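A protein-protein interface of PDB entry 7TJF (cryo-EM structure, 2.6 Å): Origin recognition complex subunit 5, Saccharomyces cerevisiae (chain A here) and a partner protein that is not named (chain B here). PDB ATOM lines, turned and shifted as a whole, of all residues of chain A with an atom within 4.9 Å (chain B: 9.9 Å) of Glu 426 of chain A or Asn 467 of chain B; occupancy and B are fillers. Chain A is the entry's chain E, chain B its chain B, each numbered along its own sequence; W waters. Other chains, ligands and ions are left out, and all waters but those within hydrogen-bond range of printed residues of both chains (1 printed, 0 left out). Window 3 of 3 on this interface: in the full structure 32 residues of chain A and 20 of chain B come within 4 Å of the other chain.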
ATOM      1  N   GLN A 422     -29.345 -30.125 -14.171  1.00  0.00           N
ATOM      2  CA  GLN A 422     -28.885 -28.764 -13.921  1.00  0.00           C
ATOM      3  C   GLN A 422     -27.678 -28.743 -12.989  1.00  0.00           C
ATOM      4  O   GLN A 422     -26.731 -27.978 -13.213  1.00  0.00           O
ATOM      5  CB  GLN A 422     -30.026 -27.931 -13.342  1.00  0.00           C
ATOM      6  CG  GLN A 422     -29.741 -26.447 -13.284  1.00  0.00           C
ATOM      7  CD  GLN A 422     -30.861 -25.669 -12.633  1.00  0.00           C
ATOM      8  OE1 GLN A 422     -32.034 -26.011 -12.776  1.00  0.00           O
ATOM      9  NE2 GLN A 422     -30.505 -24.618 -11.906  1.00  0.00           N
ATOM     10  N   ASN A 423     -27.694 -29.582 -11.944  1.00  0.00           N
ATOM     11  CA  ASN A 423     -26.548 -29.708 -11.049  1.00  0.00           C
ATOM     12  C   ASN A 423     -25.332 -30.269 -11.778  1.00  0.00           C
ATOM     13  O   ASN A 423     -24.204 -29.829 -11.537  1.00  0.00           O
ATOM     14  CB  ASN A 423     -26.914 -30.596  -9.859  1.00  0.00           C
ATOM     15  CG  ASN A 423     -27.605 -29.830  -8.751  1.00  0.00           C
ATOM     16  OD1 ASN A 423     -27.089 -28.833  -8.253  1.00  0.00           O
ATOM     17  ND2 ASN A 423     -28.792 -30.282  -8.373  1.00  0.00           N
ATOM     18  N   LEU A 424     -25.550 -31.238 -12.672  1.00  0.00           N
ATOM     19  CA  LEU A 424     -24.461 -31.801 -13.464  1.00  0.00           C
ATOM     20  C   LEU A 424     -23.860 -30.764 -14.413  1.00  0.00           C
ATOM     21  O   LEU A 424     -22.636 -30.693 -14.575  1.00  0.00           O
ATOM     22  CB  LEU A 424     -24.977 -33.011 -14.240  1.00  0.00           C
ATOM     23  CG  LEU A 424     -24.003 -33.878 -15.035  1.00  0.00           C
ATOM     24  CD1 LEU A 424     -22.725 -34.150 -14.249  1.00  0.00           C
ATOM     25  CD2 LEU A 424     -24.688 -35.172 -15.421  1.00  0.00           C
ATOM     26  N   SER A 425     -24.712 -29.948 -15.041  1.00  0.00           N
ATOM     27  CA  SER A 425     -24.232 -28.884 -15.919  1.00  0.00           C
ATOM     28  C   SER A 425     -23.486 -27.809 -15.135  1.00  0.00           C
ATOM     29  O   SER A 425     -22.501 -27.242 -15.624  1.00  0.00           O
ATOM     30  CB  SER A 425     -25.406 -28.284 -16.693  1.00  0.00           C
ATOM     31  OG  SER A 425     -24.964 -27.487 -17.777  1.00  0.00           O
ATOM     32  N   GLU A 426     -23.949 -27.514 -13.915  1.00  0.00           N
ATOM     33  CA  GLU A 426     -23.230 -26.593 -13.037  1.00  0.00           C
ATOM     34  C   GLU A 426     -21.874 -27.156 -12.628  1.00  0.00           C
ATOM     35  O   GLU A 426     -20.891 -26.414 -12.526  1.00  0.00           O
ATOM     36  CB  GLU A 426     -24.082 -26.277 -11.803  1.00  0.00           C
ATOM     37  CG  GLU A 426     -23.464 -25.292 -10.799  1.00  0.00           C
ATOM     38  CD  GLU A 426     -23.652 -23.818 -11.155  1.00  0.00           C
ATOM     39  OE1 GLU A 426     -23.822 -23.474 -12.343  1.00  0.00           O
ATOM     40  OE2 GLU A 426     -23.626 -22.991 -10.221  1.00  0.00           O
ATOM     41  N   LEU A 427     -21.805 -28.467 -12.380  1.00  0.00           N
ATOM     42  CA  LEU A 427     -20.526 -29.107 -12.088  1.00  0.00           C
ATOM     43  C   LEU A 427     -19.592 -29.080 -13.292  1.00  0.00           C
ATOM     44  O   LEU A 427     -18.369 -29.007 -13.124  1.00  0.00           O
ATOM     45  CB  LEU A 427     -20.741 -30.551 -11.634  1.00  0.00           C
ATOM     46  CG  LEU A 427     -21.292 -30.826 -10.235  1.00  0.00           C
ATOM     47  CD1 LEU A 427     -21.439 -32.322 -10.026  1.00  0.00           C
ATOM     48  CD2 LEU A 427     -20.413 -30.214  -9.164  1.00  0.00           C
ATOM     49  N   HIS A 428     -20.140 -29.145 -14.506  1.00  0.00           N
ATOM     50  CA  HIS A 428     -19.284 -29.045 -15.684  1.00  0.00           C
ATOM     51  C   HIS A 428     -18.786 -27.620 -15.901  1.00  0.00           C
ATOM     52  O   HIS A 428     -17.630 -27.420 -16.291  1.00  0.00           O
ATOM     53  CB  HIS A 428     -20.004 -29.536 -16.934  1.00  0.00           C
ATOM     54  CG  HIS A 428     -19.168 -29.431 -18.172  1.00  0.00           C
ATOM     55  ND1 HIS A 428     -19.393 -28.483 -19.146  1.00  0.00           N
ATOM     56  CD2 HIS A 428     -18.087 -30.136 -18.577  1.00  0.00           C
ATOM     57  CE1 HIS A 428     -18.496 -28.619 -20.105  1.00  0.00           C
ATOM     58  NE2 HIS A 428     -17.693 -29.616 -19.785  1.00  0.00           N
ATOM     59  N   THR A 429     -19.634 -26.616 -15.667  1.00  0.00           N
ATOM     60  CA  THR A 429     -19.180 -25.243 -15.864  1.00  0.00           C
ATOM     61  C   THR A 429     -18.270 -24.753 -14.742  1.00  0.00           C
ATOM     62  O   THR A 429     -17.616 -23.719 -14.906  1.00  0.00           O
ATOM     63  CB  THR A 429     -20.371 -24.286 -16.034  1.00  0.00           C
ATOM     64  OG1 THR A 429     -19.912 -23.057 -16.610  1.00  0.00           O
ATOM     65  CG2 THR A 429     -21.034 -23.976 -14.710  1.00  0.00           C
ATOM     66  N   LEU A 430     -18.202 -25.465 -13.623  1.00  0.00           N
ATOM     67  CA  LEU A 430     -17.217 -25.186 -12.590  1.00  0.00           C
ATOM     68  C   LEU A 430     -15.928 -25.971 -12.789  1.00  0.00           C
ATOM     69  O   LEU A 430     -14.967 -25.738 -12.048  1.00  0.00           O
ATOM     70  CB  LEU A 430     -17.802 -25.490 -11.207  1.00  0.00           C
ATOM     71  CG  LEU A 430     -18.843 -24.496 -10.691  1.00  0.00           C
ATOM     72  CD1 LEU A 430     -19.313 -24.880  -9.301  1.00  0.00           C
ATOM     73  CD2 LEU A 430     -18.286 -23.081 -10.702  1.00  0.00           C
ATOM     74  N   SER B 442     -30.776 -17.511 -24.066  1.00  0.00           N
ATOM     75  CA  SER B 442     -31.103 -17.288 -22.658  1.00  0.00           C
ATOM     76  C   SER B 442     -31.040 -15.807 -22.293  1.00  0.00           C
ATOM     77  O   SER B 442     -31.891 -15.310 -21.535  1.00  0.00           O
ATOM     78  CB  SER B 442     -30.177 -18.113 -21.764  1.00  0.00           C
ATOM     79  OG  SER B 442     -28.816 -17.909 -22.092  1.00  0.00           O
ATOM     80  N   PRO B 462     -32.093 -31.217 -20.775  1.00  0.00           N
ATOM     81  CA  PRO B 462     -31.768 -30.406 -19.582  1.00  0.00           C
ATOM     82  C   PRO B 462     -30.300 -30.412 -19.159  1.00  0.00           C
ATOM     83  O   PRO B 462     -29.934 -29.625 -18.276  1.00  0.00           O
ATOM     84  CB  PRO B 462     -32.652 -31.019 -18.490  1.00  0.00           C
ATOM     85  CG  PRO B 462     -33.786 -31.553 -19.211  1.00  0.00           C
ATOM     86  CD  PRO B 462     -33.199 -32.143 -20.443  1.00  0.00           C
ATOM     87  N   LEU B 463     -29.450 -31.252 -19.755  1.00  0.00           N
ATOM     88  CA  LEU B 463     -28.010 -31.147 -19.548  1.00  0.00           C
ATOM     89  C   LEU B 463     -27.420 -29.890 -20.182  1.00  0.00           C
ATOM     90  O   LEU B 463     -26.307 -29.495 -19.823  1.00  0.00           O
ATOM     91  CB  LEU B 463     -27.327 -32.400 -20.103  1.00  0.00           C
ATOM     92  CG  LEU B 463     -25.863 -32.735 -19.838  1.00  0.00           C
ATOM     93  CD1 LEU B 463     -25.667 -33.143 -18.400  1.00  0.00           C
ATOM     94  CD2 LEU B 463     -25.414 -33.835 -20.784  1.00  0.00           C
ATOM     95  N   LEU B 464     -28.146 -29.239 -21.098  1.00  0.00           N
ATOM     96  CA  LEU B 464     -27.617 -28.059 -21.771  1.00  0.00           C
ATOM     97  C   LEU B 464     -27.567 -26.827 -20.873  1.00  0.00           C
ATOM     98  O   LEU B 464     -26.840 -25.881 -21.189  1.00  0.00           O
ATOM     99  CB  LEU B 464     -28.450 -27.746 -23.016  1.00  0.00           C
ATOM    100  CG  LEU B 464     -28.436 -28.786 -24.138  1.00  0.00           C
ATOM    101  CD1 LEU B 464     -29.471 -28.448 -25.201  1.00  0.00           C
ATOM    102  CD2 LEU B 464     -27.050 -28.906 -24.751  1.00  0.00           C
ATOM    103  N   TRP B 465     -28.309 -26.809 -19.769  1.00  0.00           N
ATOM    104  CA  TRP B 465     -28.541 -25.585 -19.009  1.00  0.00           C
ATOM    105  C   TRP B 465     -28.028 -25.736 -17.585  1.00  0.00           C
ATOM    106  O   TRP B 465     -28.501 -26.598 -16.838  1.00  0.00           O
ATOM    107  CB  TRP B 465     -30.029 -25.229 -19.014  1.00  0.00           C
ATOM    108  CG  TRP B 465     -30.653 -25.398 -20.365  1.00  0.00           C
ATOM    109  CD1 TRP B 465     -30.213 -24.868 -21.543  1.00  0.00           C
ATOM    110  CD2 TRP B 465     -31.824 -26.155 -20.680  1.00  0.00           C
ATOM    111  NE1 TRP B 465     -31.036 -25.247 -22.570  1.00  0.00           N
ATOM    112  CE2 TRP B 465     -32.035 -26.038 -22.068  1.00  0.00           C
ATOM    113  CE3 TRP B 465     -32.717 -26.919 -19.924  1.00  0.00           C
ATOM    114  CZ2 TRP B 465     -33.098 -26.658 -22.713  1.00  0.00           C
ATOM    115  CZ3 TRP B 465     -33.770 -27.532 -20.565  1.00  0.00           C
ATOM    116  CH2 TRP B 465     -33.950 -27.402 -21.946  1.00  0.00           C
ATOM    117  N   ASP B 466     -27.082 -24.879 -17.207  1.00  0.00           N
ATOM    118  CA  ASP B 466     -26.581 -24.798 -15.844  1.00  0.00           C
ATOM    119  C   ASP B 466     -27.478 -23.866 -15.022  1.00  0.00           C
ATOM    120  O   ASP B 466     -28.573 -23.502 -15.450  1.00  0.00           O
ATOM    121  CB  ASP B 466     -25.078 -24.455 -15.870  1.00  0.00           C
ATOM    122  CG  ASP B 466     -24.744 -23.017 -16.354  1.00  0.00           C
ATOM    123  OD1 ASP B 466     -25.500 -22.035 -16.198  1.00  0.00           O
ATOM    124  OD2 ASP B 466     -23.637 -22.873 -16.913  1.00  0.00           O
ATOM    125  N   ASN B 467     -27.012 -23.475 -13.829  1.00  0.00           N
ATOM    126  CA  ASN B 467     -27.812 -22.648 -12.924  1.00  0.00           C
ATOM    127  C   ASN B 467     -28.067 -21.256 -13.496  1.00  0.00           C
ATOM    128  O   ASN B 467     -29.180 -20.727 -13.380  1.00  0.00           O
ATOM    129  CB  ASN B 467     -27.116 -22.539 -11.568  1.00  0.00           C
ATOM    130  CG  ASN B 467     -27.388 -23.726 -10.667  1.00  0.00           C
ATOM    131  OD1 ASN B 467     -27.981 -24.716 -11.085  1.00  0.00           O
ATOM    132  ND2 ASN B 467     -26.944 -23.632  -9.422  1.00  0.00           N
ATOM    133  N   MET B 468     -27.052 -20.658 -14.130  1.00  0.00           N
ATOM    134  CA  MET B 468     -27.196 -19.322 -14.699  1.00  0.00           C
ATOM    135  C   MET B 468     -28.128 -19.329 -15.906  1.00  0.00           C
ATOM    136  O   MET B 468     -28.987 -18.447 -16.040  1.00  0.00           O
ATOM    137  CB  MET B 468     -25.817 -18.793 -15.101  1.00  0.00           C
ATOM    138  CG  MET B 468     -25.685 -17.297 -15.395  1.00  0.00           C
ATOM    139  SD  MET B 468     -26.166 -16.181 -14.056  1.00  0.00           S
ATOM    140  CE  MET B 468     -27.809 -15.692 -14.544  1.00  0.00           C
ATOM    141  N   LYS B 469     -28.012 -20.347 -16.761  1.00  0.00           N
ATOM    142  CA  LYS B 469     -28.878 -20.447 -17.928  1.00  0.00           C
ATOM    143  C   LYS B 469     -30.293 -20.868 -17.554  1.00  0.00           C
ATOM    144  O   LYS B 469     -31.245 -20.461 -18.227  1.00  0.00           O
ATOM    145  CB  LYS B 469     -28.282 -21.423 -18.944  1.00  0.00           C
ATOM    146  CG  LYS B 469     -27.360 -20.770 -19.959  1.00  0.00           C
ATOM    147  CD  LYS B 469     -26.903 -21.762 -21.019  1.00  0.00           C
ATOM    148  CE  LYS B 469     -25.571 -21.351 -21.630  1.00  0.00           C
ATOM    149  NZ  LYS B 469     -24.414 -21.931 -20.895  1.00  0.00           N
ATOM    150  N   ALA B 470     -30.457 -21.667 -16.495  1.00  0.00           N
ATOM    151  CA  ALA B 470     -31.800 -21.983 -16.021  1.00  0.00           C
ATOM    152  C   ALA B 470     -32.461 -20.777 -15.373  1.00  0.00           C
ATOM    153  O   ALA B 470     -33.683 -20.619 -15.468  1.00  0.00           O
ATOM    154  CB  ALA B 470     -31.772 -23.152 -15.037  1.00  0.00           C
ATOM    155  N   GLN B 471     -31.676 -19.933 -14.698  1.00  0.00           N
ATOM    156  CA  GLN B 471     -32.210 -18.692 -14.149  1.00  0.00           C
ATOM    157  C   GLN B 471     -32.638 -17.740 -15.260  1.00  0.00           C
ATOM    158  O   GLN B 471     -33.697 -17.109 -15.179  1.00  0.00           O
ATOM    159  CB  GLN B 471     -31.167 -18.027 -13.254  1.00  0.00           C
ATOM    160  CG  GLN B 471     -31.751 -17.341 -12.047  1.00  0.00           C
ATOM    161  CD  GLN B 471     -30.976 -16.108 -11.637  1.00  0.00           C
ATOM    162  OE1 GLN B 471     -30.327 -15.468 -12.457  1.00  0.00           O
ATOM    163  NE2 GLN B 471     -31.045 -15.766 -10.359  1.00  0.00           N
ATOM    164  N   ASN B 472     -31.818 -17.628 -16.309  1.00  0.00           N
ATOM    165  CA  ASN B 472     -32.116 -16.687 -17.385  1.00  0.00           C
ATOM    166  C   ASN B 472     -33.258 -17.176 -18.268  1.00  0.00           C
ATOM    167  O   ASN B 472     -34.074 -16.372 -18.733  1.00  0.00           O
ATOM    168  CB  ASN B 472     -30.862 -16.436 -18.217  1.00  0.00           C
ATOM    169  CG  ASN B 472     -29.888 -15.510 -17.528  1.00  0.00           C
ATOM    170  OD1 ASN B 472     -30.246 -14.810 -16.584  1.00  0.00           O
ATOM    171  ND2 ASN B 472     -28.648 -15.502 -17.994  1.00  0.00           N
ATOM    172  N   TYR B 473     -33.329 -18.486 -18.515  1.00  0.00           N
ATOM    173  CA  TYR B 473     -34.377 -19.031 -19.371  1.00  0.00           C
ATOM    174  C   TYR B 473     -35.746 -18.947 -18.707  1.00  0.00           C
ATOM    175  O   TYR B 473     -36.732 -18.609 -19.372  1.00  0.00           O
ATOM    176  CB  TYR B 473     -34.051 -20.476 -19.739  1.00  0.00           C
ATOM    177  CG  TYR B 473     -33.349 -20.650 -21.066  1.00  0.00           C
ATOM    178  CD1 TYR B 473     -33.796 -19.990 -22.208  1.00  0.00           C
ATOM    179  CD2 TYR B 473     -32.247 -21.488 -21.182  1.00  0.00           C
ATOM    180  CE1 TYR B 473     -33.164 -20.161 -23.424  1.00  0.00           C
ATOM    181  CE2 TYR B 473     -31.605 -21.660 -22.390  1.00  0.00           C
ATOM    182  CZ  TYR B 473     -32.064 -20.995 -23.507  1.00  0.00           C
ATOM    183  OH  TYR B 473     -31.421 -21.173 -24.707  1.00  0.00           O
ATOM    184  N   ASN B 474     -35.812 -19.239 -17.398  1.00  0.00           N
ATOM    185  CA  ASN B 474     -37.032 -19.174 -16.577  1.00  0.00           C
ATOM    186  C   ASN B 474     -38.142 -20.061 -17.147  1.00  0.00           C
ATOM    187  O   ASN B 474     -39.251 -19.608 -17.435  1.00  0.00           O
ATOM    188  CB  ASN B 474     -37.501 -17.723 -16.403  1.00  0.00           C
ATOM    189  CG  ASN B 474     -38.438 -17.546 -15.228  1.00  0.00           C
ATOM    190  OD1 ASN B 474     -38.327 -18.238 -14.220  1.00  0.00           O
ATOM    191  ND2 ASN B 474     -39.365 -16.605 -15.352  1.00  0.00           N
ATOM    192  N   PHE B 475     -37.824 -21.338 -17.321  1.00  0.00           N
ATOM    193  CA  PHE B 475     -38.703 -22.258 -18.026  1.00  0.00           C
ATOM    194  C   PHE B 475     -39.864 -22.716 -17.153  1.00  0.00           C
ATOM    195  O   PHE B 475     -39.700 -22.988 -15.960  1.00  0.00           O
ATOM    196  CB  PHE B 475     -37.926 -23.484 -18.501  1.00  0.00           C
ATOM    197  CG  PHE B 475     -37.157 -23.268 -19.768  1.00  0.00           C
ATOM    198  CD1 PHE B 475     -37.707 -22.543 -20.815  1.00  0.00           C
ATOM    199  CD2 PHE B 475     -35.887 -23.803 -19.919  1.00  0.00           C
ATOM    200  CE1 PHE B 475     -37.000 -22.346 -21.984  1.00  0.00           C
ATOM    201  CE2 PHE B 475     -35.175 -23.612 -21.088  1.00  0.00           C
ATOM    202  CZ  PHE B 475     -35.733 -22.880 -22.120  1.00  0.00           C
HETATM  203  O   HOH W   1     -30.935 -21.593 -11.224  1.00  0.00           O
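Water W1 lies within hydrogen-bond range of O of Asn 467 of chain B (2.9 Å) and NE2 of Gln 422 of chain A (3.1 Å).
Of the printed residues of chain B, Leu 424 of chain A touches Leu 463 (3.7 Å). Ser 425 of chain A touches three residues of chain B. Glu 426 of chain A touches just these residues of chain B: Asp 466 (3.8 Å) and Asn 467 (3.5 Å). No residue of chain B comes within 4 Å of Leu 427 of chain A. Thr 429 of chain A touches just one residue of chain B: Asp 466. Printed residues of chain A within 4 Å of Asp 466 of chain B: Gln 422 (3.8 Å), Ser 425 (3.4 Å), Glu 426 (3.8 Å) and Thr 429 (3.6 Å). Of the printed residues of chain A, Asn 467 of chain B touches Gln 422 (2.7 Å) and Glu 426 (3.5 Å). Of the printed residues of chain A, Ala 470 of chain B touches Gln 422 (3.6 Å). The nearest residue of chain B that does not touch Glu 426 of chain A is Met 468 of chain B (4.6 Å). The nearest printed residue of chain A that does not touch Asn 467 of chain B is Asn 423 of chain A (4.9 Å).
Gln 422 of chain A touches Trp 465 of chain B. Gln 422 of chain A touches Asp 466 of chain B (CG to O, 3.8 Å). Gln 422 of chain A touches Ala 470 of chain B (CD to CB, 3.6 Å). CD1 of Leu 463 of chain B touches CD2 of Leu 424 of chain A, at 3.7 Å. Ser 425 of chain A touches Trp 465 of chain B (CB to O, 3.5 Å). Asp 466 of chain B touches Glu 426 of chain A. Thr 429 of chain A touches Asp 466 of chain B (CG2 to OD2, 3.6 Å).
The side-chain carboxylate (OD1) of Asp 466 of chain B sits at hydrogen-bond distance from the backbone NH (N) of Met 468 of chain B (2.9 Å). The side-chain carboxylate (OD1) of Asp 466 of chain B sits at hydrogen-bond distance from the backbone NH (N) of Lys 469 of chain B, 3.1 Å away.
Of the 9 printed residues of chain A, 5 touch a printed residue of chain B. Hydrophobic or aromatic side chains of chain A that line the printed part of chain B: Leu 424. Of the 15 printed residues of chain B, 5 touch a printed residue of chain A. Hydrophobic or aromatic side chains of chain B that line the printed part of chain A: Leu 463 and Ala 470. Along chain B the printed residues that touch a printed residue of chain A span positions 463 to 470. Among the printed residues, 11 pairs touch across the chains. Among the printed residues, no Asp or Glu carboxylate lies within 4 Å of a Lys or Arg side-chain nitrogen of the other chain.
OG of Ser 425 of chain A sits at hydrogen-bond distance from O of Leu 463 of chain B (3.2 Å). The backbone NH (N) of Asp 466 of chain B sits at hydrogen-bond distance from the side-chain hydroxyl (OG) of Ser 425 of chain A (3.4 Å). OD1 of Asn 467 of chain B lies within hydrogen-bond range of NE2 of Gln 422 of chain A. The side-chain amide nitrogen (ND2) of Asn 467 of chain B lies within hydrogen-bond range of the side-chain carboxylate (OE2) of Glu 426 of chain A, at 3.5 Å.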
